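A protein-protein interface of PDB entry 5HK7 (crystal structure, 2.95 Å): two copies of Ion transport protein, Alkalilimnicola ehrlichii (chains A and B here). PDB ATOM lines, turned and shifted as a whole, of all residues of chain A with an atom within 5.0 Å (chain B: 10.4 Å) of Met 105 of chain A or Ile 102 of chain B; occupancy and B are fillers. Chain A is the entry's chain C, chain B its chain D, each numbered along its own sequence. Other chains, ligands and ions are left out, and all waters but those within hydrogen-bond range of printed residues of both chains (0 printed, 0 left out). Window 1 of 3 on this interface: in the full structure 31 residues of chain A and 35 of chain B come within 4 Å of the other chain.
Ser 104 of chain A touches Ile 102 of chain B, but with the chains exchanged Ile 102 of chain A does not touch Ser 104 of chain B (13.3 Å). Met 105 of chain B touches its own counterpart, Met 105 of chain A. Ala 108 of chain A touches Ile 102 of chain B, but with the chains exchanged Ile 102 of chain A does not touch Ala 108 of chain B (16.1 Å). Ala 108 of chain A touches Trp 110 of chain B, but with the chains exchanged Trp 110 of chain A does not touch Ala 108 of chain B (12.2 Å). 11 positions are printed for both chains.
The backbone carbonyl oxygen (O) of Met 105 of chain B sits at hydrogen-bond distance from the backbone NH (N) of Trp 110 of chain B (3.3 Å).
Hydrophobic or aromatic side chains of chain B that line the printed part of chain A: Ile 98, Ile 101, Ile 102, Met 105 and Trp 110. Printed residues of chain A that touch a printed residue of chain B: Ile 101, Ser 104, Met 105, Ala 108 and His 109. Hydrophobic or aromatic side chains of chain A within 4 Å of the printed part of chain B: Ile 101, Met 105, Ala 108 and His 109.
No residue of chain B comes within 4 Å of Ile 102 of chain A. Met 105 of chain A touches just these residues of chain B: Ile 102 and Met 105. Ser 107 of chain A touches none of the printed residues of chain B. Of chain B, only Ile 102 (3.8 Å) and Trp 110 (3.98 Å) come within 4 Å of Ala 108 of chain A. Glu 111 of chain A touches none of the printed residues of chain B. Of the printed residues of chain A, Ile 98 of chain B touches Ile 101 and Ser 104. Of the printed residues of chain A, Ile 101 of chain B touches Ile 101 (3.6 Å). Of chain A, only Ser 104 (3.9 Å), Met 105 (3.7 Å) and Ala 108 (3.8 Å) come within 4 Å of Ile 102 of chain B. Of the printed residues of chain A, Met 105 of chain B touches Met 105 (2.8 Å). Gln 106 of chain B touches none of the printed residues of chain A. Of the printed residues of chain A, Trp 110 of chain B touches Ala 108 (3.98 Å) and His 109 (3.4 Å). The nearest residue of chain B that does not touch Met 105 of chain A is Trp 110 of chain B (4.5 Å). The nearest printed residue of chain B that does not touch His 109 of chain A is Gln 106 of chain B (4.5 Å).
CG1 of Ile 98 of chain B touches CD1 of Ile 101 of chain A, at 3.6 Å. CD1 of Ile 101 of chain A touches CD1 of Ile 101 of chain B (3.6 Å). OG of Ser 104 of chain A touches CG2 of Ile 98 of chain B (3.5 Å). Ile 102 of chain B touches Ser 104 of chain A (CD1 to C, 3.9 Å). Ile 102 of chain B touches Met 105 of chain A (CD1 to CA, 3.7 Å). Met 105 of chain B touches Met 105 of chain A. Ile 102 of chain B touches Ala 108 of chain A. Ala 108 of chain A touches Trp 110 of chain B (CB to CZ3, 3.98 Å). His 109 of chain A touches Trp 110 of chain B (CG to CD2, 3.4 Å).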
ATOM      1  N   ILE A 101      34.025  -0.510  24.222  1.00  0.00           N
ATOM      2  CA  ILE A 101      32.676  -0.688  24.814  1.00  0.00           C
ATOM      3  C   ILE A 101      32.803  -1.372  26.145  1.00  0.00           C
ATOM      4  O   ILE A 101      32.158  -0.984  27.096  1.00  0.00           O
ATOM      5  CB  ILE A 101      31.650  -1.433  23.924  1.00  0.00           C
ATOM      6  CG1 ILE A 101      30.262  -0.909  24.240  1.00  0.00           C
ATOM      7  CG2 ILE A 101      31.648  -2.943  24.149  1.00  0.00           C
ATOM      8  CD1 ILE A 101      29.552  -0.363  23.030  1.00  0.00           C
ATOM      9  N   ILE A 102      33.691  -2.360  26.186  1.00  0.00           N
ATOM     10  CA  ILE A 102      33.976  -3.191  27.356  1.00  0.00           C
ATOM     11  C   ILE A 102      34.678  -2.430  28.470  1.00  0.00           C
ATOM     12  O   ILE A 102      34.188  -2.404  29.567  1.00  0.00           O
ATOM     13  CB  ILE A 102      34.754  -4.476  26.943  1.00  0.00           C
ATOM     14  CG1 ILE A 102      33.763  -5.622  26.695  1.00  0.00           C
ATOM     15  CG2 ILE A 102      35.913  -4.801  27.885  1.00  0.00           C
ATOM     16  CD1 ILE A 102      34.456  -6.914  26.382  1.00  0.00           C
ATOM     17  N   GLU A 103      35.806  -1.809  28.187  1.00  0.00           N
ATOM     18  CA  GLU A 103      36.461  -0.990  29.175  1.00  0.00           C
ATOM     19  C   GLU A 103      35.517   0.154  29.561  1.00  0.00           C
ATOM     20  O   GLU A 103      35.684   0.819  30.588  1.00  0.00           O
ATOM     21  CB  GLU A 103      37.775  -0.468  28.614  1.00  0.00           C
ATOM     22  CG  GLU A 103      38.321   0.745  29.340  1.00  0.00           C
ATOM     23  CD  GLU A 103      39.317   0.373  30.413  1.00  0.00           C
ATOM     24  OE1 GLU A 103      39.796  -0.778  30.377  1.00  0.00           O
ATOM     25  OE2 GLU A 103      39.614   1.224  31.286  1.00  0.00           O
ATOM     26  N   SER A 104      34.507   0.379  28.742  1.00  0.00           N
ATOM     27  CA  SER A 104      33.551   1.394  29.102  1.00  0.00           C
ATOM     28  C   SER A 104      32.609   0.880  30.155  1.00  0.00           C
ATOM     29  O   SER A 104      32.261   1.614  31.059  1.00  0.00           O
ATOM     30  CB  SER A 104      32.762   1.885  27.900  1.00  0.00           C
ATOM     31  OG  SER A 104      32.615   3.289  27.969  1.00  0.00           O
ATOM     32  N   MET A 105      32.199  -0.384  30.042  1.00  0.00           N
ATOM     33  CA  MET A 105      31.309  -0.991  31.041  1.00  0.00           C
ATOM     34  C   MET A 105      32.030  -1.077  32.370  1.00  0.00           C
ATOM     35  O   MET A 105      31.505  -0.655  33.394  1.00  0.00           O
ATOM     36  CB  MET A 105      30.858  -2.359  30.626  1.00  0.00           C
ATOM     37  CG  MET A 105      30.383  -2.381  29.219  1.00  0.00           C
ATOM     38  SD  MET A 105      29.075  -3.589  29.039  1.00  0.00           S
ATOM     39  CE  MET A 105      29.899  -4.676  27.879  1.00  0.00           C
ATOM     40  N   GLN A 106      33.259  -1.570  32.341  1.00  0.00           N
ATOM     41  CA  GLN A 106      34.050  -1.631  33.542  1.00  0.00           C
ATOM     42  C   GLN A 106      33.950  -0.371  34.376  1.00  0.00           C
ATOM     43  O   GLN A 106      33.489  -0.408  35.527  1.00  0.00           O
ATOM     44  CB  GLN A 106      35.501  -1.897  33.222  1.00  0.00           C
ATOM     45  CG  GLN A 106      36.332  -2.155  34.456  1.00  0.00           C
ATOM     46  CD  GLN A 106      36.563  -3.635  34.684  1.00  0.00           C
ATOM     47  OE1 GLN A 106      37.309  -4.012  35.588  1.00  0.00           O
ATOM     48  NE2 GLN A 106      35.937  -4.483  33.858  1.00  0.00           N
ATOM     49  N   SER A 107      34.403   0.742  33.828  1.00  0.00           N
ATOM     50  CA  SER A 107      34.410   1.924  34.633  1.00  0.00           C
ATOM     51  C   SER A 107      32.987   2.362  35.026  1.00  0.00           C
ATOM     52  O   SER A 107      32.783   2.927  36.093  1.00  0.00           O
ATOM     53  CB  SER A 107      35.148   3.028  33.944  1.00  0.00           C
ATOM     54  OG  SER A 107      34.844   4.216  34.633  1.00  0.00           O
ATOM     55  N   ALA A 108      32.009   2.087  34.177  1.00  0.00           N
ATOM     56  CA  ALA A 108      30.627   2.443  34.495  1.00  0.00           C
ATOM     57  C   ALA A 108      30.177   1.703  35.730  1.00  0.00           C
ATOM     58  O   ALA A 108      29.770   2.311  36.693  1.00  0.00           O
ATOM     59  CB  ALA A 108      29.696   2.127  33.333  1.00  0.00           C
ATOM     60  N   HIS A 109      30.271   0.383  35.705  1.00  0.00           N
ATOM     61  CA  HIS A 109      29.452  -0.435  36.566  1.00  0.00           C
ATOM     62  C   HIS A 109      30.244  -1.563  37.183  1.00  0.00           C
ATOM     63  O   HIS A 109      30.215  -1.698  38.370  1.00  0.00           O
ATOM     64  CB  HIS A 109      28.254  -0.969  35.812  1.00  0.00           C
ATOM     65  CG  HIS A 109      27.440  -1.930  36.601  1.00  0.00           C
ATOM     66  ND1 HIS A 109      26.539  -1.520  37.559  1.00  0.00           N
ATOM     67  CD2 HIS A 109      27.372  -3.284  36.566  1.00  0.00           C
ATOM     68  CE1 HIS A 109      25.954  -2.584  38.084  1.00  0.00           C
ATOM     69  NE2 HIS A 109      26.441  -3.666  37.500  1.00  0.00           N
ATOM     70  N   TRP A 110      30.926  -2.391  36.405  1.00  0.00           N
ATOM     71  CA  TRP A 110      31.626  -3.524  36.980  1.00  0.00           C
ATOM     72  C   TRP A 110      32.721  -3.106  37.953  1.00  0.00           C
ATOM     73  O   TRP A 110      33.163  -3.881  38.781  1.00  0.00           O
ATOM     74  CB  TRP A 110      32.276  -4.332  35.903  1.00  0.00           C
ATOM     75  CG  TRP A 110      31.376  -4.888  34.849  1.00  0.00           C
ATOM     76  CD1 TRP A 110      30.012  -5.172  34.920  1.00  0.00           C
ATOM     77  CD2 TRP A 110      31.789  -5.285  33.555  1.00  0.00           C
ATOM     78  NE1 TRP A 110      29.572  -5.730  33.721  1.00  0.00           N
ATOM     79  CE2 TRP A 110      30.645  -5.805  32.873  1.00  0.00           C
ATOM     80  CE3 TRP A 110      33.023  -5.261  32.896  1.00  0.00           C
ATOM     81  CZ2 TRP A 110      30.716  -6.271  31.569  1.00  0.00           C
ATOM     82  CZ3 TRP A 110      33.092  -5.723  31.611  1.00  0.00           C
ATOM     83  CH2 TRP A 110      31.947  -6.221  30.948  1.00  0.00           C
ATOM     84  N   GLU A 111      33.166  -1.872  37.855  1.00  0.00           N
ATOM     85  CA  GLU A 111      34.166  -1.408  38.794  1.00  0.00           C
ATOM     86  C   GLU A 111      33.646  -1.628  40.197  1.00  0.00           C
ATOM     87  O   GLU A 111      34.179  -2.423  40.975  1.00  0.00           O
ATOM     88  CB  GLU A 111      34.443   0.093  38.592  1.00  0.00           C
ATOM     89  CG  GLU A 111      35.871   0.522  38.924  1.00  0.00           C
ATOM     90  CD  GLU A 111      36.880  -0.006  37.908  1.00  0.00           C
ATOM     91  OE1 GLU A 111      37.096  -1.239  37.839  1.00  0.00           O
ATOM     92  OE2 GLU A 111      37.448   0.808  37.155  1.00  0.00           O
ATOM     93  N   GLY B  13      25.277  13.983  31.268  1.00  0.00           N
ATOM     94  CA  GLY B  13      25.745  12.663  30.812  1.00  0.00           C
ATOM     95  C   GLY B  13      26.363  12.561  29.405  1.00  0.00           C
ATOM     96  O   GLY B  13      27.469  13.050  29.175  1.00  0.00           O
ATOM     97  N   ILE B  14      25.668  11.891  28.479  1.00  0.00           N
ATOM     98  CA  ILE B  14      26.047  11.826  27.060  1.00  0.00           C
ATOM     99  C   ILE B  14      25.897  13.193  26.406  1.00  0.00           C
ATOM    100  O   ILE B  14      26.774  13.657  25.687  1.00  0.00           O
ATOM    101  CB  ILE B  14      25.149  10.836  26.276  1.00  0.00           C
ATOM    102  CG1 ILE B  14      23.779  10.596  26.944  1.00  0.00           C
ATOM    103  CG2 ILE B  14      25.850   9.508  26.115  1.00  0.00           C
ATOM    104  CD1 ILE B  14      22.908  11.821  27.129  1.00  0.00           C
ATOM    105  N   ILE B  17      28.739  15.198  25.326  1.00  0.00           N
ATOM    106  CA  ILE B  17      29.323  15.133  23.964  1.00  0.00           C
ATOM    107  C   ILE B  17      28.396  15.606  22.868  1.00  0.00           C
ATOM    108  O   ILE B  17      28.812  16.353  21.994  1.00  0.00           O
ATOM    109  CB  ILE B  17      29.806  13.737  23.536  1.00  0.00           C
ATOM    110  CG1 ILE B  17      28.929  12.639  24.106  1.00  0.00           C
ATOM    111  CG2 ILE B  17      31.246  13.537  23.944  1.00  0.00           C
ATOM    112  CD1 ILE B  17      29.418  11.280  23.696  1.00  0.00           C
ATOM    113  N   LEU B  94      31.077   7.722  17.873  1.00  0.00           N
ATOM    114  CA  LEU B  94      31.315   6.402  18.389  1.00  0.00           C
ATOM    115  C   LEU B  94      30.935   6.434  19.833  1.00  0.00           C
ATOM    116  O   LEU B  94      30.153   5.611  20.280  1.00  0.00           O
ATOM    117  CB  LEU B  94      32.778   6.025  18.291  1.00  0.00           C
ATOM    118  CG  LEU B  94      33.041   4.596  18.757  1.00  0.00           C
ATOM    119  CD1 LEU B  94      32.412   3.676  17.721  1.00  0.00           C
ATOM    120  CD2 LEU B  94      34.529   4.299  18.952  1.00  0.00           C
ATOM    121  N   ASN B  95      31.489   7.408  20.553  1.00  0.00           N
ATOM    122  CA  ASN B  95      31.270   7.537  21.989  1.00  0.00           C
ATOM    123  C   ASN B  95      29.874   7.885  22.370  1.00  0.00           C
ATOM    124  O   ASN B  95      29.376   7.374  23.354  1.00  0.00           O
ATOM    125  CB  ASN B  95      32.198   8.547  22.621  1.00  0.00           C
ATOM    126  CG  ASN B  95      33.637   8.113  22.564  1.00  0.00           C
ATOM    127  OD1 ASN B  95      33.993   7.047  22.032  1.00  0.00           O
ATOM    128  ND2 ASN B  95      34.490   8.951  23.096  1.00  0.00           N
ATOM    129  N   LEU B  96      29.234   8.767  21.622  1.00  0.00           N
ATOM    130  CA  LEU B  96      27.857   9.076  21.920  1.00  0.00           C
ATOM    131  C   LEU B  96      27.072   7.781  21.856  1.00  0.00           C
ATOM    132  O   LEU B  96      26.076   7.596  22.532  1.00  0.00           O
ATOM    133  CB  LEU B  96      27.296  10.092  20.934  1.00  0.00           C
ATOM    134  CG  LEU B  96      25.791  10.288  21.102  1.00  0.00           C
ATOM    135  CD1 LEU B  96      25.592  11.410  22.094  1.00  0.00           C
ATOM    136  CD2 LEU B  96      25.044  10.532  19.796  1.00  0.00           C
ATOM    137  N   PHE B  97      27.532   6.875  21.024  1.00  0.00           N
ATOM    138  CA  PHE B  97      26.799   5.663  20.811  1.00  0.00           C
ATOM    139  C   PHE B  97      26.998   4.794  22.051  1.00  0.00           C
ATOM    140  O   PHE B  97      26.017   4.302  22.605  1.00  0.00           O
ATOM    141  CB  PHE B  97      27.302   5.020  19.515  1.00  0.00           C
ATOM    142  CG  PHE B  97      26.791   3.626  19.246  1.00  0.00           C
ATOM    143  CD1 PHE B  97      25.424   3.368  19.142  1.00  0.00           C
ATOM    144  CD2 PHE B  97      27.702   2.556  19.037  1.00  0.00           C
ATOM    145  CE1 PHE B  97      24.973   2.071  18.868  1.00  0.00           C
ATOM    146  CE2 PHE B  97      27.253   1.263  18.764  1.00  0.00           C
ATOM    147  CZ  PHE B  97      25.887   1.025  18.672  1.00  0.00           C
ATOM    148  N   ILE B  98      28.253   4.629  22.491  1.00  0.00           N
ATOM    149  CA  ILE B  98      28.588   3.781  23.633  1.00  0.00           C
ATOM    150  C   ILE B  98      27.861   4.347  24.818  1.00  0.00           C
ATOM    151  O   ILE B  98      27.089   3.644  25.465  1.00  0.00           O
ATOM    152  CB  ILE B  98      30.089   3.824  23.972  1.00  0.00           C
ATOM    153  CG1 ILE B  98      30.877   3.031  22.963  1.00  0.00           C
ATOM    154  CG2 ILE B  98      30.374   3.185  25.314  1.00  0.00           C
ATOM    155  CD1 ILE B  98      32.315   2.860  23.387  1.00  0.00           C
ATOM    156  N   GLY B  99      28.118   5.621  25.103  1.00  0.00           N
ATOM    157  CA  GLY B  99      27.470   6.286  26.198  1.00  0.00           C
ATOM    158  C   GLY B  99      25.983   5.968  26.231  1.00  0.00           C
ATOM    159  O   GLY B  99      25.403   5.816  27.292  1.00  0.00           O
ATOM    160  N   ILE B 100      25.346   5.850  25.080  1.00  0.00           N
ATOM    161  CA  ILE B 100      23.939   5.509  25.112  1.00  0.00           C
ATOM    162  C   ILE B 100      23.714   4.051  25.412  1.00  0.00           C
ATOM    163  O   ILE B 100      22.804   3.739  26.164  1.00  0.00           O
ATOM    164  CB  ILE B 100      23.178   5.897  23.848  1.00  0.00           C
ATOM    165  CG1 ILE B 100      23.147   7.411  23.723  1.00  0.00           C
ATOM    166  CG2 ILE B 100      21.745   5.400  23.930  1.00  0.00           C
ATOM    167  CD1 ILE B 100      22.912   7.863  22.297  1.00  0.00           C
ATOM    168  N   ILE B 101      24.527   3.153  24.870  1.00  0.00           N
ATOM    169  CA  ILE B 101      24.429   1.775  25.349  1.00  0.00           C
ATOM    170  C   ILE B 101      24.620   1.628  26.872  1.00  0.00           C
ATOM    171  O   ILE B 101      23.736   1.088  27.536  1.00  0.00           O
ATOM    172  CB  ILE B 101      25.391   0.832  24.639  1.00  0.00           C
ATOM    173  CG1 ILE B 101      25.328   1.036  23.145  1.00  0.00           C
ATOM    174  CG2 ILE B 101      25.026  -0.610  24.946  1.00  0.00           C
ATOM    175  CD1 ILE B 101      25.971  -0.120  22.411  1.00  0.00           C
ATOM    176  N   ILE B 102      25.756   2.097  27.408  1.00  0.00           N
ATOM    177  CA  ILE B 102      25.979   2.130  28.860  1.00  0.00           C
ATOM    178  C   ILE B 102      24.696   2.632  29.540  1.00  0.00           C
ATOM    179  O   ILE B 102      24.018   1.901  30.256  1.00  0.00           O
ATOM    180  CB  ILE B 102      27.156   3.061  29.241  1.00  0.00           C
ATOM    181  CG1 ILE B 102      28.502   2.483  28.826  1.00  0.00           C
ATOM    182  CG2 ILE B 102      27.246   3.280  30.719  1.00  0.00           C
ATOM    183  CD1 ILE B 102      28.781   1.058  29.223  1.00  0.00           C
ATOM    184  N   GLU B 103      24.357   3.880  29.281  1.00  0.00           N
ATOM    185  CA  GLU B 103      23.204   4.501  29.886  1.00  0.00           C
ATOM    186  C   GLU B 103      21.940   3.685  29.691  1.00  0.00           C
ATOM    187  O   GLU B 103      21.109   3.607  30.574  1.00  0.00           O
ATOM    188  CB  GLU B 103      22.972   5.837  29.238  1.00  0.00           C
ATOM    189  CG  GLU B 103      21.946   6.664  29.967  1.00  0.00           C
ATOM    190  CD  GLU B 103      22.605   7.779  30.723  1.00  0.00           C
ATOM    191  OE1 GLU B 103      23.846   7.716  30.895  1.00  0.00           O
ATOM    192  OE2 GLU B 103      21.884   8.717  31.135  1.00  0.00           O
ATOM    193  N   SER B 104      21.776   3.103  28.517  1.00  0.00           N
ATOM    194  CA  SER B 104      20.613   2.282  28.273  1.00  0.00           C
ATOM    195  C   SER B 104      20.610   1.062  29.199  1.00  0.00           C
ATOM    196  O   SER B 104      19.633   0.800  29.900  1.00  0.00           O
ATOM    197  CB  SER B 104      20.517   1.880  26.802  1.00  0.00           C
ATOM    198  OG  SER B 104      19.150   1.901  26.410  1.00  0.00           O
ATOM    199  N   MET B 105      21.719   0.341  29.242  1.00  0.00           N
ATOM    200  CA  MET B 105      21.796  -0.824  30.097  1.00  0.00           C
ATOM    201  C   MET B 105      21.956  -0.516  31.608  1.00  0.00           C
ATOM    202  O   MET B 105      21.710  -1.379  32.446  1.00  0.00           O
ATOM    203  CB  MET B 105      22.859  -1.780  29.571  1.00  0.00           C
ATOM    204  CG  MET B 105      24.299  -1.321  29.701  1.00  0.00           C
ATOM    205  SD  MET B 105      25.227  -2.707  29.012  1.00  0.00           S
ATOM    206  CE  MET B 105      26.819  -1.938  28.826  1.00  0.00           C
ATOM    207  N   GLN B 106      22.321   0.712  31.962  1.00  0.00           N
ATOM    208  CA  GLN B 106      22.209   1.144  33.360  1.00  0.00           C
ATOM    209  C   GLN B 106      20.782   1.167  33.791  1.00  0.00           C
ATOM    210  O   GLN B 106      20.503   1.183  34.961  1.00  0.00           O
ATOM    211  CB  GLN B 106      22.783   2.539  33.604  1.00  0.00           C
ATOM    212  CG  GLN B 106      22.679   3.039  35.051  1.00  0.00           C
ATOM    213  CD  GLN B 106      23.908   2.673  35.875  1.00  0.00           C
ATOM    214  OE1 GLN B 106      23.797   2.012  36.913  1.00  0.00           O
ATOM    215  NE2 GLN B 106      25.092   3.085  35.405  1.00  0.00           N
ATOM    216  N   SER B 107      19.865   1.183  32.853  1.00  0.00           N
ATOM    217  CA  SER B 107      18.492   1.274  33.236  1.00  0.00           C
ATOM    218  C   SER B 107      17.867  -0.099  33.214  1.00  0.00           C
ATOM    219  O   SER B 107      17.189  -0.488  34.167  1.00  0.00           O
ATOM    220  CB  SER B 107      17.750   2.198  32.311  1.00  0.00           C
ATOM    221  OG  SER B 107      16.373   1.887  32.321  1.00  0.00           O
ATOM    222  N   ALA B 108      18.119  -0.830  32.135  1.00  0.00           N
ATOM    223  CA  ALA B 108      17.498  -2.119  31.905  1.00  0.00           C
ATOM    224  C   ALA B 108      17.738  -3.001  33.111  1.00  0.00           C
ATOM    225  O   ALA B 108      16.845  -3.686  33.612  1.00  0.00           O
ATOM    226  CB  ALA B 108      18.108  -2.750  30.675  1.00  0.00           C
ATOM    227  N   HIS B 109      18.965  -2.947  33.592  1.00  0.00           N
ATOM    228  CA  HIS B 109      19.428  -3.929  34.499  1.00  0.00           C
ATOM    229  C   HIS B 109      20.050  -3.299  35.691  1.00  0.00           C
ATOM    230  O   HIS B 109      19.608  -3.541  36.801  1.00  0.00           O
ATOM    231  CB  HIS B 109      20.491  -4.740  33.856  1.00  0.00           C
ATOM    232  CG  HIS B 109      20.834  -5.958  34.632  1.00  0.00           C
ATOM    233  ND1 HIS B 109      19.894  -6.906  34.959  1.00  0.00           N
ATOM    234  CD2 HIS B 109      22.009  -6.383  35.156  1.00  0.00           C
ATOM    235  CE1 HIS B 109      20.481  -7.875  35.641  1.00  0.00           C
ATOM    236  NE2 HIS B 109      21.765  -7.584  35.771  1.00  0.00           N
ATOM    237  N   TRP B 110      21.135  -2.567  35.475  1.00  0.00           N
ATOM    238  CA  TRP B 110      22.063  -2.339  36.552  1.00  0.00           C
ATOM    239  C   TRP B 110      21.408  -1.568  37.670  1.00  0.00           C
ATOM    240  O   TRP B 110      21.730  -1.770  38.823  1.00  0.00           O
ATOM    241  CB  TRP B 110      23.249  -1.538  36.111  1.00  0.00           C
ATOM    242  CG  TRP B 110      24.100  -2.207  35.143  1.00  0.00           C
ATOM    243  CD1 TRP B 110      24.204  -3.559  34.897  1.00  0.00           C
ATOM    244  CD2 TRP B 110      25.012  -1.561  34.254  1.00  0.00           C
ATOM    245  NE1 TRP B 110      25.141  -3.788  33.907  1.00  0.00           N
ATOM    246  CE2 TRP B 110      25.646  -2.576  33.495  1.00  0.00           C
ATOM    247  CE3 TRP B 110      25.364  -0.219  34.027  1.00  0.00           C
ATOM    248  CZ2 TRP B 110      26.600  -2.284  32.530  1.00  0.00           C
ATOM    249  CZ3 TRP B 110      26.306   0.062  33.073  1.00  0.00           C
ATOM    250  CH2 TRP B 110      26.912  -0.965  32.333  1.00  0.00           C
ATOM    251  N   GLU B 111      20.495  -0.668  37.346  1.00  0.00           N
ATOM    252  CA  GLU B 111      19.959   0.164  38.396  1.00  0.00           C
ATOM    253  C   GLU B 111      19.092  -0.665  39.270  1.00  0.00           C
ATOM    254  O   GLU B 111      19.182  -0.580  40.501  1.00  0.00           O
ATOM    255  CB  GLU B 111      19.141   1.297  37.833  1.00  0.00           C
ATOM    256  CG  GLU B 111      19.925   2.587  37.880  1.00  0.00           C
ATOM    257  CD  GLU B 111      19.039   3.787  38.005  1.00  0.00           C
ATOM    258  OE1 GLU B 111      17.864   3.594  38.405  1.00  0.00           O
ATOM    259  OE2 GLU B 111      19.528   4.901  37.699  1.00  0.00           O
